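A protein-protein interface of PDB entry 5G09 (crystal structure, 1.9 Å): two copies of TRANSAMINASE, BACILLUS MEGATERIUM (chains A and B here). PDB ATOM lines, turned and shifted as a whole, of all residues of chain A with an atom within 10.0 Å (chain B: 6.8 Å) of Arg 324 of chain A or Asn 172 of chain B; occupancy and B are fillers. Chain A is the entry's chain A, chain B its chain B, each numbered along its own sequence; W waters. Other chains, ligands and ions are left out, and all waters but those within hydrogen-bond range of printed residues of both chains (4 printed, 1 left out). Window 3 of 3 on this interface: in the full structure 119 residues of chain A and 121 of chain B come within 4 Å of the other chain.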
ATOM      1  N   LEU A 134     -12.042  -0.527  16.966  1.00  0.00           N
ATOM      2  CA  LEU A 134     -11.055   0.368  17.574  1.00  0.00           C
ATOM      3  C   LEU A 134     -10.526   1.447  16.585  1.00  0.00           C
ATOM      4  O   LEU A 134     -10.379   2.626  16.948  1.00  0.00           O
ATOM      5  CB  LEU A 134      -9.886  -0.441  18.169  1.00  0.00           C
ATOM      6  CG  LEU A 134     -10.193  -1.178  19.483  1.00  0.00           C
ATOM      7  CD1 LEU A 134      -9.124  -2.240  19.719  1.00  0.00           C
ATOM      8  CD2 LEU A 134     -10.358  -0.269  20.710  1.00  0.00           C
ATOM      9  N   ALA A 318      -0.624   1.541  11.127  1.00  0.00           N
ATOM     10  CA  ALA A 318       0.042   2.762  11.621  1.00  0.00           C
ATOM     11  C   ALA A 318      -0.704   3.298  12.857  1.00  0.00           C
ATOM     12  O   ALA A 318      -0.074   3.689  13.823  1.00  0.00           O
ATOM     13  CB  ALA A 318       0.140   3.851  10.524  1.00  0.00           C
ATOM     14  N   PHE A 319      -2.041   3.282  12.819  1.00  0.00           N
ATOM     15  CA  PHE A 319      -2.862   3.660  13.985  1.00  0.00           C
ATOM     16  C   PHE A 319      -2.620   2.739  15.197  1.00  0.00           C
ATOM     17  O   PHE A 319      -2.337   3.210  16.312  1.00  0.00           O
ATOM     18  CB  PHE A 319      -4.353   3.677  13.574  1.00  0.00           C
ATOM     19  CG  PHE A 319      -5.314   3.816  14.731  1.00  0.00           C
ATOM     20  CD1 PHE A 319      -5.815   2.674  15.387  1.00  0.00           C
ATOM     21  CD2 PHE A 319      -5.737   5.072  15.152  1.00  0.00           C
ATOM     22  CE1 PHE A 319      -6.715   2.801  16.441  1.00  0.00           C
ATOM     23  CE2 PHE A 319      -6.626   5.207  16.222  1.00  0.00           C
ATOM     24  CZ  PHE A 319      -7.115   4.067  16.861  1.00  0.00           C
ATOM     25  N   MET A 320      -2.708   1.434  14.988  1.00  0.00           N
ATOM     26  CA  MET A 320      -2.554   0.474  16.083  1.00  0.00           C
ATOM     27  C   MET A 320      -1.180   0.575  16.745  1.00  0.00           C
ATOM     28  O   MET A 320      -1.061   0.528  17.988  1.00  0.00           O
ATOM     29  CB  MET A 320      -2.820  -0.946  15.601  1.00  0.00           C
ATOM     30  CG  MET A 320      -4.271  -1.206  15.195  1.00  0.00           C
ATOM     31  SD  MET A 320      -5.487  -1.109  16.544  1.00  0.00           S
ATOM     32  CE  MET A 320      -4.951  -2.447  17.623  1.00  0.00           C
ATOM     33  N   ASP A 321      -0.168   0.756  15.901  1.00  0.00           N
ATOM     34  CA  ASP A 321       1.227   0.984  16.310  1.00  0.00           C
ATOM     35  C   ASP A 321       1.420   2.140  17.285  1.00  0.00           C
ATOM     36  O   ASP A 321       2.363   2.111  18.070  1.00  0.00           O
ATOM     37  CB  ASP A 321       2.102   1.240  15.084  1.00  0.00           C
ATOM     38  CG  ASP A 321       2.602  -0.045  14.423  1.00  0.00           C
ATOM     39  OD1 ASP A 321       2.345  -1.193  14.887  1.00  0.00           O
ATOM     40  OD2 ASP A 321       3.278   0.115  13.408  1.00  0.00           O
ATOM     41  N   LYS A 322       0.513   3.111  17.272  1.00  0.00           N
ATOM     42  CA  LYS A 322       0.625   4.273  18.180  1.00  0.00           C
ATOM     43  C   LYS A 322       0.126   4.021  19.607  1.00  0.00           C
ATOM     44  O   LYS A 322       0.263   4.871  20.477  1.00  0.00           O
ATOM     45  CB  LYS A 322      -0.113   5.463  17.581  1.00  0.00           C
ATOM     46  CG  LYS A 322       0.594   5.989  16.343  1.00  0.00           C
ATOM     47  CD  LYS A 322      -0.314   6.940  15.595  1.00  0.00           C
ATOM     48  CE  LYS A 322       0.339   7.402  14.299  1.00  0.00           C
ATOM     49  NZ  LYS A 322      -0.496   8.491  13.768  1.00  0.00           N
ATOM     50  N   HIS A 323      -0.466   2.860  19.852  1.00  0.00           N
ATOM     51  CA  HIS A 323      -1.063   2.586  21.151  1.00  0.00           C
ATOM     52  C   HIS A 323      -0.522   1.308  21.755  1.00  0.00           C
ATOM     53  O   HIS A 323       0.149   0.527  21.073  1.00  0.00           O
ATOM     54  CB  HIS A 323      -2.568   2.479  21.021  1.00  0.00           C
ATOM     55  CG  HIS A 323      -3.198   3.661  20.363  1.00  0.00           C
ATOM     56  ND1 HIS A 323      -3.519   3.680  19.027  1.00  0.00           N
ATOM     57  CD2 HIS A 323      -3.563   4.864  20.853  1.00  0.00           C
ATOM     58  CE1 HIS A 323      -4.084   4.834  18.726  1.00  0.00           C
ATOM     59  NE2 HIS A 323      -4.112   5.575  19.814  1.00  0.00           N
ATOM     60  N   ARG A 324      -0.771   1.134  23.050  1.00  0.00           N
ATOM     61  CA  ARG A 324      -0.512  -0.122  23.743  1.00  0.00           C
ATOM     62  C   ARG A 324      -1.807  -0.934  23.688  1.00  0.00           C
ATOM     63  O   ARG A 324      -2.839  -0.514  24.233  1.00  0.00           O
ATOM     64  CB  ARG A 324      -0.095   0.153  25.188  1.00  0.00           C
ATOM     65  CG  ARG A 324       1.262   0.872  25.302  1.00  0.00           C
ATOM     66  CD  ARG A 324       1.620   1.117  26.753  1.00  0.00           C
ATOM     67  NE  ARG A 324       2.976   1.626  26.929  1.00  0.00           N
ATOM     68  CZ  ARG A 324       3.379   2.321  27.994  1.00  0.00           C
ATOM     69  NH1 ARG A 324       2.529   2.625  28.981  1.00  0.00           N
ATOM     70  NH2 ARG A 324       4.635   2.724  28.062  1.00  0.00           N
ATOM     71  N   TRP A 325      -1.759  -2.068  22.999  1.00  0.00           N
ATOM     72  CA  TRP A 325      -2.951  -2.897  22.820  1.00  0.00           C
ATOM     73  C   TRP A 325      -3.008  -4.035  23.834  1.00  0.00           C
ATOM     74  O   TRP A 325      -2.137  -4.926  23.835  1.00  0.00           O
ATOM     75  CB  TRP A 325      -2.963  -3.450  21.393  1.00  0.00           C
ATOM     76  CG  TRP A 325      -4.267  -4.123  20.955  1.00  0.00           C
ATOM     77  CD1 TRP A 325      -5.506  -3.973  21.483  1.00  0.00           C
ATOM     78  CD2 TRP A 325      -4.403  -4.986  19.834  1.00  0.00           C
ATOM     79  NE1 TRP A 325      -6.429  -4.729  20.766  1.00  0.00           N
ATOM     80  CE2 TRP A 325      -5.766  -5.357  19.747  1.00  0.00           C
ATOM     81  CE3 TRP A 325      -3.486  -5.514  18.902  1.00  0.00           C
ATOM     82  CZ2 TRP A 325      -6.247  -6.222  18.752  1.00  0.00           C
ATOM     83  CZ3 TRP A 325      -3.969  -6.361  17.902  1.00  0.00           C
ATOM     84  CH2 TRP A 325      -5.344  -6.703  17.838  1.00  0.00           C
ATOM     85  N   GLU A 326      -4.027  -4.012  24.688  1.00  0.00           N
ATOM     86  CA  GLU A 326      -4.072  -4.884  25.872  1.00  0.00           C
ATOM     87  C   GLU A 326      -4.733  -6.221  25.569  1.00  0.00           C
ATOM     88  O   GLU A 326      -5.716  -6.592  26.217  1.00  0.00           O
ATOM     89  CB  GLU A 326      -4.801  -4.164  27.024  1.00  0.00           C
ATOM     90  CG  GLU A 326      -4.123  -2.869  27.452  1.00  0.00           C
ATOM     91  CD  GLU A 326      -4.831  -2.195  28.608  1.00  0.00           C
ATOM     92  OE1 GLU A 326      -6.044  -1.915  28.455  1.00  0.00           O
ATOM     93  OE2 GLU A 326      -4.188  -1.946  29.671  1.00  0.00           O
ATOM     94  N   SER A 327      -4.196  -6.931  24.562  1.00  0.00           N
ATOM     95  CA  SER A 327      -4.825  -8.163  24.085  1.00  0.00           C
ATOM     96  C   SER A 327      -3.790  -9.273  24.101  1.00  0.00           C
ATOM     97  O   SER A 327      -2.696  -9.133  23.524  1.00  0.00           O
ATOM     98  CB  SER A 327      -5.408  -7.988  22.686  1.00  0.00           C
ATOM     99  OG  SER A 327      -6.401  -8.985  22.429  1.00  0.00           O
ATOM    100  N   VAL A 328      -4.126 -10.363  24.783  1.00  0.00           N
ATOM    101  CA  VAL A 328      -3.259 -11.521  24.805  1.00  0.00           C
ATOM    102  C   VAL A 328      -4.050 -12.773  24.512  1.00  0.00           C
ATOM    103  O   VAL A 328      -5.188 -12.923  24.982  1.00  0.00           O
ATOM    104  CB  VAL A 328      -2.487 -11.643  26.157  1.00  0.00           C
ATOM    105  CG1 VAL A 328      -3.442 -11.736  27.359  1.00  0.00           C
ATOM    106  CG2 VAL A 328      -1.506 -12.820  26.122  1.00  0.00           C
ATOM    107  N   ARG B  23       1.767  -5.088  17.194  1.00  0.00           N
ATOM    108  CA  ARG B  23       2.241  -4.946  18.577  1.00  0.00           C
ATOM    109  C   ARG B  23       1.123  -5.239  19.589  1.00  0.00           C
ATOM    110  O   ARG B  23      -0.037  -4.868  19.364  1.00  0.00           O
ATOM    111  CB  ARG B  23       2.735  -3.500  18.817  1.00  0.00           C
ATOM    112  CG  ARG B  23       3.922  -3.074  17.975  1.00  0.00           C
ATOM    113  CD  ARG B  23       5.247  -3.625  18.527  1.00  0.00           C
ATOM    114  NE  ARG B  23       5.490  -5.050  18.246  1.00  0.00           N
ATOM    115  CZ  ARG B  23       5.908  -5.549  17.075  1.00  0.00           C
ATOM    116  NH1 ARG B  23       6.145  -4.758  16.032  1.00  0.00           N
ATOM    117  NH2 ARG B  23       6.095  -6.868  16.946  1.00  0.00           N
ATOM    118  N   THR B  24       1.479  -5.868  20.705  1.00  0.00           N
ATOM    119  CA  THR B  24       0.594  -5.900  21.864  1.00  0.00           C
ATOM    120  C   THR B  24       1.341  -5.376  23.083  1.00  0.00           C
ATOM    121  O   THR B  24       2.531  -5.610  23.220  1.00  0.00           O
ATOM    122  CB  THR B  24       0.005  -7.316  22.095  1.00  0.00           C
ATOM    123  OG1 THR B  24       1.051  -8.294  22.154  1.00  0.00           O
ATOM    124  CG2 THR B  24      -0.938  -7.702  20.937  1.00  0.00           C
ATOM    125  N   PHE B  25       0.651  -4.633  23.948  1.00  0.00           N
ATOM    126  CA  PHE B  25       1.236  -4.107  25.201  1.00  0.00           C
ATOM    127  C   PHE B  25       2.348  -3.039  25.062  1.00  0.00           C
ATOM    128  O   PHE B  25       2.576  -2.276  25.991  1.00  0.00           O
ATOM    129  CB  PHE B  25       1.661  -5.257  26.154  1.00  0.00           C
ATOM    130  CG  PHE B  25       0.520  -6.165  26.527  1.00  0.00           C
ATOM    131  CD1 PHE B  25      -0.425  -5.768  27.479  1.00  0.00           C
ATOM    132  CD2 PHE B  25       0.355  -7.406  25.889  1.00  0.00           C
ATOM    133  CE1 PHE B  25      -1.493  -6.599  27.808  1.00  0.00           C
ATOM    134  CE2 PHE B  25      -0.724  -8.235  26.216  1.00  0.00           C
ATOM    135  CZ  PHE B  25      -1.649  -7.841  27.167  1.00  0.00           C
ATOM    136  N   SER B  26       3.000  -2.959  23.903  1.00  0.00           N
ATOM    137  CA  SER B  26       4.037  -1.953  23.629  1.00  0.00           C
ATOM    138  C   SER B  26       3.608  -1.151  22.421  1.00  0.00           C
ATOM    139  O   SER B  26       3.045  -1.716  21.475  1.00  0.00           O
ATOM    140  CB  SER B  26       5.369  -2.622  23.255  1.00  0.00           C
ATOM    141  OG  SER B  26       5.808  -3.530  24.249  1.00  0.00           O
ATOM    142  N   THR B  27       3.890   0.146  22.402  1.00  0.00           N
ATOM    143  CA  THR B  27       3.751   0.888  21.146  1.00  0.00           C
ATOM    144  C   THR B  27       4.906   0.433  20.240  1.00  0.00           C
ATOM    145  O   THR B  27       5.914  -0.121  20.719  1.00  0.00           O
ATOM    146  CB  THR B  27       3.901   2.418  21.328  1.00  0.00           C
ATOM    147  OG1 THR B  27       5.247   2.694  21.768  1.00  0.00           O
ATOM    148  CG2 THR B  27       2.888   2.966  22.371  1.00  0.00           C
ATOM    149  N   GLU B  30       8.324   2.184  21.269  1.00  0.00           N
ATOM    150  CA  GLU B  30       9.058   1.747  22.449  1.00  0.00           C
ATOM    151  C   GLU B  30       9.449   0.280  22.346  1.00  0.00           C
ATOM    152  O   GLU B  30      10.151  -0.238  23.206  1.00  0.00           O
ATOM    153  CB  GLU B  30       8.211   1.972  23.709  1.00  0.00           C
ATOM    154  CG  GLU B  30       7.084   0.949  23.904  1.00  0.00           C
ATOM    155  CD  GLU B  30       6.058   1.391  24.922  1.00  0.00           C
ATOM    156  OE1 GLU B  30       6.412   2.116  25.878  1.00  0.00           O
ATOM    157  OE2 GLU B  30       4.882   1.023  24.777  1.00  0.00           O
ATOM    158  N   GLY B 167      -8.569  -3.520  24.727  1.00  0.00           N
ATOM    159  CA  GLY B 167      -8.722  -2.099  24.388  1.00  0.00           C
ATOM    160  C   GLY B 167      -7.371  -1.443  24.166  1.00  0.00           C
ATOM    161  O   GLY B 167      -6.321  -2.095  24.258  1.00  0.00           O
ATOM    162  N   LEU B 168      -7.410  -0.145  23.850  1.00  0.00           N
ATOM    163  CA  LEU B 168      -6.199   0.654  23.629  1.00  0.00           C
ATOM    164  C   LEU B 168      -5.936   1.615  24.755  1.00  0.00           C
ATOM    165  O   LEU B 168      -6.857   2.273  25.266  1.00  0.00           O
ATOM    166  CB  LEU B 168      -6.287   1.453  22.332  1.00  0.00           C
ATOM    167  CG  LEU B 168      -6.424   0.647  21.030  1.00  0.00           C
ATOM    168  CD1 LEU B 168      -6.604   1.620  19.876  1.00  0.00           C
ATOM    169  CD2 LEU B 168      -5.263  -0.322  20.783  1.00  0.00           C
ATOM    170  N   VAL B 169      -4.677   1.703  25.146  1.00  0.00           N
ATOM    171  CA  VAL B 169      -4.266   2.739  26.082  1.00  0.00           C
ATOM    172  C   VAL B 169      -3.063   3.515  25.528  1.00  0.00           C
ATOM    173  O   VAL B 169      -2.435   3.101  24.535  1.00  0.00           O
ATOM    174  CB  VAL B 169      -4.032   2.185  27.522  1.00  0.00           C
ATOM    175  CG1 VAL B 169      -5.335   1.633  28.113  1.00  0.00           C
ATOM    176  CG2 VAL B 169      -2.908   1.147  27.544  1.00  0.00           C
ATOM    177  N   GLY B 170      -2.744   4.629  26.184  1.00  0.00           N
ATOM    178  CA  GLY B 170      -1.681   5.519  25.726  1.00  0.00           C
ATOM    179  C   GLY B 170      -0.321   5.056  26.200  1.00  0.00           C
ATOM    180  O   GLY B 170      -0.208   4.119  26.992  1.00  0.00           O
ATOM    181  N   GLU B 171       0.711   5.734  25.721  1.00  0.00           N
ATOM    182  CA  GLU B 171       2.081   5.404  26.081  1.00  0.00           C
ATOM    183  C   GLU B 171       2.500   6.324  27.202  1.00  0.00           C
ATOM    184  O   GLU B 171       2.732   7.503  26.954  1.00  0.00           O
ATOM    185  CB  GLU B 171       2.974   5.658  24.872  1.00  0.00           C
ATOM    186  CG  GLU B 171       4.463   5.464  25.081  1.00  0.00           C
ATOM    187  CD  GLU B 171       5.204   5.898  23.843  1.00  0.00           C
ATOM    188  OE1 GLU B 171       5.465   7.114  23.729  1.00  0.00           O
ATOM    189  OE2 GLU B 171       5.458   5.041  22.957  1.00  0.00           O
ATOM    190  N   ASN B 172       2.583   5.794  28.422  1.00  0.00           N
ATOM    191  CA  ASN B 172       2.905   6.586  29.619  1.00  0.00           C
ATOM    192  C   ASN B 172       2.014   7.798  29.809  1.00  0.00           C
ATOM    193  O   ASN B 172       2.457   8.847  30.255  1.00  0.00           O
ATOM    194  CB  ASN B 172       4.374   6.997  29.608  1.00  0.00           C
ATOM    195  CG  ASN B 172       5.268   5.842  29.242  1.00  0.00           C
ATOM    196  OD1 ASN B 172       5.189   4.755  29.843  1.00  0.00           O
ATOM    197  ND2 ASN B 172       6.087   6.045  28.215  1.00  0.00           N
ATOM    198  N   SER B 173       0.749   7.633  29.453  1.00  0.00           N
ATOM    199  CA  SER B 173      -0.272   8.632  29.678  1.00  0.00           C
ATOM    200  C   SER B 173      -1.555   7.883  30.021  1.00  0.00           C
ATOM    201  O   SER B 173      -1.895   6.880  29.381  1.00  0.00           O
ATOM    202  CB  SER B 173      -0.438   9.520  28.436  1.00  0.00           C
ATOM    203  OG  SER B 173      -1.741  10.079  28.350  1.00  0.00           O
ATOM    204  N   GLU B 174      -2.231   8.329  31.075  1.00  0.00           N
ATOM    205  CA  GLU B 174      -3.597   7.883  31.310  1.00  0.00           C
ATOM    206  C   GLU B 174      -4.496   9.051  30.934  1.00  0.00           C
ATOM    207  O   GLU B 174      -5.002   9.785  31.776  1.00  0.00           O
ATOM    208  CB  GLU B 174      -3.796   7.311  32.724  1.00  0.00           C
ATOM    209  CG  GLU B 174      -3.213   5.901  32.842  1.00  0.00           C
ATOM    210  CD  GLU B 174      -3.438   5.224  34.187  1.00  0.00           C
ATOM    211  OE1 GLU B 174      -3.026   5.792  35.225  1.00  0.00           O
ATOM    212  OE2 GLU B 174      -3.998   4.098  34.206  1.00  0.00           O
ATOM    213  N   SER B 175      -4.622   9.237  29.627  1.00  0.00           N
ATOM    214  CA  SER B 175      -5.396  10.313  29.044  1.00  0.00           C
ATOM    215  C   SER B 175      -6.139   9.712  27.871  1.00  0.00           C
ATOM    216  O   SER B 175      -7.342   9.475  27.957  1.00  0.00           O
ATOM    217  CB  SER B 175      -4.488  11.444  28.560  1.00  0.00           C
ATOM    218  OG  SER B 175      -3.491  11.741  29.521  1.00  0.00           O
ATOM    219  N   PHE B 176      -5.418   9.458  26.778  1.00  0.00           N
ATOM    220  CA  PHE B 176      -5.996   8.753  25.637  1.00  0.00           C
ATOM    221  C   PHE B 176      -6.105   7.247  25.917  1.00  0.00           C
ATOM    222  O   PHE B 176      -5.102   6.584  26.179  1.00  0.00           O
ATOM    223  CB  PHE B 176      -5.290   9.087  24.298  1.00  0.00           C
ATOM    224  CG  PHE B 176      -3.783   9.240  24.390  1.00  0.00           C
ATOM    225  CD1 PHE B 176      -3.206  10.344  25.029  1.00  0.00           C
ATOM    226  CD2 PHE B 176      -2.936   8.304  23.784  1.00  0.00           C
ATOM    227  CE1 PHE B 176      -1.825  10.485  25.095  1.00  0.00           C
ATOM    228  CE2 PHE B 176      -1.552   8.444  23.848  1.00  0.00           C
ATOM    229  CZ  PHE B 176      -0.998   9.534  24.504  1.00  0.00           C
ATOM    230  N   THR B 409      -4.399   0.390  34.530  1.00  0.00           N
ATOM    231  CA  THR B 409      -4.317   0.109  33.097  1.00  0.00           C
ATOM    232  C   THR B 409      -2.835   0.152  32.640  1.00  0.00           C
ATOM    233  O   THR B 409      -1.975   0.683  33.359  1.00  0.00           O
ATOM    234  CB  THR B 409      -5.147   1.105  32.252  1.00  0.00           C
ATOM    235  OG1 THR B 409      -4.401   2.301  32.035  1.00  0.00           O
ATOM    236  CG2 THR B 409      -6.506   1.446  32.915  1.00  0.00           C
ATOM    237  N   HIS B 410      -2.545  -0.382  31.452  1.00  0.00           N
ATOM    238  CA  HIS B 410      -1.188  -0.317  30.887  1.00  0.00           C
ATOM    239  C   HIS B 410      -0.784   1.078  30.344  1.00  0.00           C
ATOM    240  O   HIS B 410       0.275   1.226  29.754  1.00  0.00           O
ATOM    241  CB  HIS B 410      -0.988  -1.410  29.816  1.00  0.00           C
ATOM    242  CG  HIS B 410      -1.040  -2.797  30.371  1.00  0.00           C
ATOM    243  ND1 HIS B 410      -2.192  -3.552  30.375  1.00  0.00           N
ATOM    244  CD2 HIS B 410      -0.078  -3.565  30.950  1.00  0.00           C
ATOM    245  CE1 HIS B 410      -1.938  -4.732  30.932  1.00  0.00           C
ATOM    246  NE2 HIS B 410      -0.665  -4.762  31.295  1.00  0.00           N
ATOM    247  N   GLY B 411      -1.640   2.085  30.545  1.00  0.00           N
ATOM    248  CA  GLY B 411      -1.304   3.483  30.243  1.00  0.00           C
ATOM    249  C   GLY B 411      -0.234   4.010  31.183  1.00  0.00           C
ATOM    250  O   GLY B 411       0.505   4.919  30.833  1.00  0.00           O
ATOM    251  N   MET B 412      -0.143   3.426  32.376  1.00  0.00           N
ATOM    252  CA  MET B 412       0.887   3.776  33.365  1.00  0.00           C
ATOM    253  C   MET B 412       2.310   3.693  32.787  1.00  0.00           C
ATOM    254  O   MET B 412       2.570   2.927  31.857  1.00  0.00           O
ATOM    255  CB  MET B 412       0.811   2.818  34.555  1.00  0.00           C
ATOM    256  CG  MET B 412      -0.251   3.133  35.576  1.00  0.00           C
ATOM    257  SD  MET B 412       0.118   2.279  37.124  1.00  0.00           S
ATOM    258  CE  MET B 412       1.513   3.242  37.743  1.00  0.00           C
ATOM    259  N   ASN B 413       3.226   4.463  33.358  1.00  0.00           N
ATOM    260  CA  ASN B 413       4.643   4.297  33.068  1.00  0.00           C
ATOM    261  C   ASN B 413       5.182   3.097  33.854  1.00  0.00           C
ATOM    262  O   ASN B 413       5.060   3.052  35.089  1.00  0.00           O
ATOM    263  CB  ASN B 413       5.417   5.569  33.441  1.00  0.00           C
ATOM    264  CG  ASN B 413       6.792   5.638  32.795  1.00  0.00           C
ATOM    265  OD1 ASN B 413       7.552   4.658  32.761  1.00  0.00           O
ATOM    266  ND2 ASN B 413       7.127   6.815  32.281  1.00  0.00           N
ATOM    267  N   PRO B 414       5.787   2.125  33.147  1.00  0.00           N
ATOM    268  CA  PRO B 414       6.437   0.987  33.803  1.00  0.00           C
ATOM    269  C   PRO B 414       7.451   1.360  34.905  1.00  0.00           C
ATOM    270  O   PRO B 414       7.646   0.570  35.828  1.00  0.00           O
ATOM    271  CB  PRO B 414       7.157   0.276  32.656  1.00  0.00           C
ATOM    272  CG  PRO B 414       6.391   0.660  31.439  1.00  0.00           C
ATOM    273  CD  PRO B 414       5.864   2.040  31.675  1.00  0.00           C
ATOM    274  N   ASN B 415       8.096   2.524  34.816  1.00  0.00           N
ATOM    275  CA  ASN B 415       9.079   2.891  35.847  1.00  0.00           C
ATOM    276  C   ASN B 415       8.450   3.253  37.213  1.00  0.00           C
ATOM    277  O   ASN B 415       9.153   3.510  38.202  1.00  0.00           O
ATOM    278  CB  ASN B 415      10.043   3.967  35.347  1.00  0.00           C
ATOM    279  CG  ASN B 415       9.356   5.281  35.032  1.00  0.00           C
ATOM    280  OD1 ASN B 415       8.373   5.667  35.659  1.00  0.00           O
ATOM    281  ND2 ASN B 415       9.892   5.987  34.057  1.00  0.00           N
HETATM  282  O   HOH W   1       0.422  -2.795  15.862  1.00  0.00           O
HETATM  283  O   HOH W   2      -0.272 -10.381  23.127  1.00  0.00           O
HETATM  284  O   HOH W   3      -1.000  -2.411  18.239  1.00  0.00           O
HETATM  285  O   HOH W   4      -8.304  -3.416  27.636  1.00  0.00           O
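OE1 of Glu 30 of chain B is in salt-bridge range of NH2 of Arg 324 of chain A, 2.9 Å away. N of Arg 324 of chain A sits at hydrogen-bond distance from O of Val 169 of chain B, at 3.0 Å. OD1 of Asn 172 of chain B is in hydrogen-bond range of NH2 of Arg 324 of chain A, at 2.8 Å. The backbone carbonyl oxygen of His 410 of chain B is in hydrogen-bond range of the guanidinium group of Arg 324 of chain A (2.8 Å). The backbone carbonyl oxygen (O) of Met 412 of chain B is in hydrogen-bond range of the guanidinium group (NH1) of Arg 324 of chain A, at 2.9 Å. The backbone carbonyl oxygen (O) of Trp 325 of chain A sits at hydrogen-bond distance from the backbone NH (N) of Phe 25 of chain B (2.8 Å). O of Gly 167 of chain B is in hydrogen-bond range of N of Glu 326 of chain A (3.0 Å). The side-chain carboxylate of Glu 326 of chain A is in hydrogen-bond range of a ring nitrogen (ND1) of His 410 of chain B.
A ring nitrogen (ND1) of His 323 of chain A lies within hydrogen-bond range of the backbone carbonyl oxygen of Phe 319 of chain A. OE2 of Glu 171 of chain B sits at hydrogen-bond distance from OG1 of Thr 27 of chain B, 2.6 Å away. O of Phe 176 of chain B is in hydrogen-bond range of N of Gly 170 of chain B, 3.1 Å away. The backbone NH (N) of Asn 172 of chain B sits close to the backbone carbonyl oxygen (O) of Gly 411 of chain B (3.3 Å). The side-chain carboxylate (OE2) of Glu 174 of chain B sits at hydrogen-bond distance from the side-chain hydroxyl (OG1) of Thr 409 of chain B, 2.8 Å away. The backbone NH (N) of Gly 411 of chain B sits close to the side-chain hydroxyl (OG1) of Thr 409 of chain B, 3.1 Å away.
Thr 27 of chain B touches Asp 321 of chain A. CG2 of Thr 27 of chain B touches O of Lys 322 of chain A, at 3.8 Å. Arg 324 of chain A touches Leu 168 of chain B. Gly 170 of chain B touches Arg 324 of chain A (O to CD, 3.5 Å). Arg 324 of chain A touches Pro 414 of chain B (NH2 to CD, 3.9 Å). Trp 325 of chain A touches Leu 168 of chain B. Phe 25 of chain B touches Glu 326 of chain A. CG2 of Thr 24 of chain B touches O of Ser 327 of chain A (3.4 Å). Phe 25 of chain B touches Ser 327 of chain A (CE2 to O, 3.5 Å). CB of Val 328 of chain A touches CE2 of Phe 25 of chain B, at 3.8 Å.
Printed residues of chain B within 4 Å of Asp 321 of chain A: Arg 23 and Thr 27. Of chain B, only Phe 25 (3.5 Å), Thr 27 (3.95 Å), Glu 30 (2.9 Å), Gly 167 (3.8 Å), Leu 168 (3.6 Å), Val 169 (3.0 Å), Gly 170 (3.5 Å), Glu 171 (3.9 Å), Asn 172 (2.8 Å), His 410 (2.8 Å), Gly 411 (3.6 Å), Met 412 (2.9 Å) and Pro 414 (3.9 Å) come within 4 Å of Arg 324 of chain A. Printed residues of chain B within 4 Å of Glu 326 of chain A: Phe 25, Gly 167, Val 169, Thr 409 and His 410. Of the printed residues of chain A, Arg 23 of chain B touches Asp 321 (3.9 Å) and Trp 325 (3.5 Å). Of the printed residues of chain A, Thr 24 of chain B touches Trp 325 (3.5 Å) and Ser 327 (3.4 Å). Val 169 of chain B touches three residues of chain A. Of chain A, only Arg 324 (3.5 Å) comes within 4 Å of Gly 170 of chain B. Glu 171 of chain B touches one residue of chain A. Asn 172 of chain B touches one residue of chain A. Phe 176 of chain B touches none of the printed residues of chain A. Printed residues of chain A within 4 Å of Gly 411 of chain B: Arg 324 (3.6 Å). No residue of chain A comes within 4 Å of Asn 413 of chain B. The nearest residue of chain A that does not touch Asn 172 of chain B is Lys 322 of chain A (8.3 Å).
Hydrophobic or aromatic side chains of chain B within 4 Å of the printed part of chain A: Phe 25, Leu 168, Val 169, His 410 and Pro 414. Hydrophobic or aromatic side chains of chain A that line the printed part of chain B: Phe 319, Met 320, His 323, Trp 325 and Val 328. Among the printed residues, Asp or Glu carboxylates within 4 Å of a Lys or Arg side-chain nitrogen of the other chain: Arg 324 of chain A with Glu 30 of chain B.
No position is printed for both chains. Of the 35 pairs that touch across the chains among the printed residues, none has its exchanged pair printed and touching as well.
Water W2 bridges OG1 of Thr 24 of chain B and O of Ser 327 of chain A. Water W1 lies within hydrogen-bond range of OD1 of Asp 321 of chain A and N of Arg 23 of chain B. Water W4 bridges the side-chain carboxylate of Glu 326 of chain A (2.8 Å) and the backbone NH of Gly 167 of chain B (2.9 Å). Water W3 lies within hydrogen-bond range of the backbone carbonyl oxygen of Arg 23 of chain B (2.9 Å) and the backbone carbonyl oxygen of Met 320 of chain A (3.0 Å).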
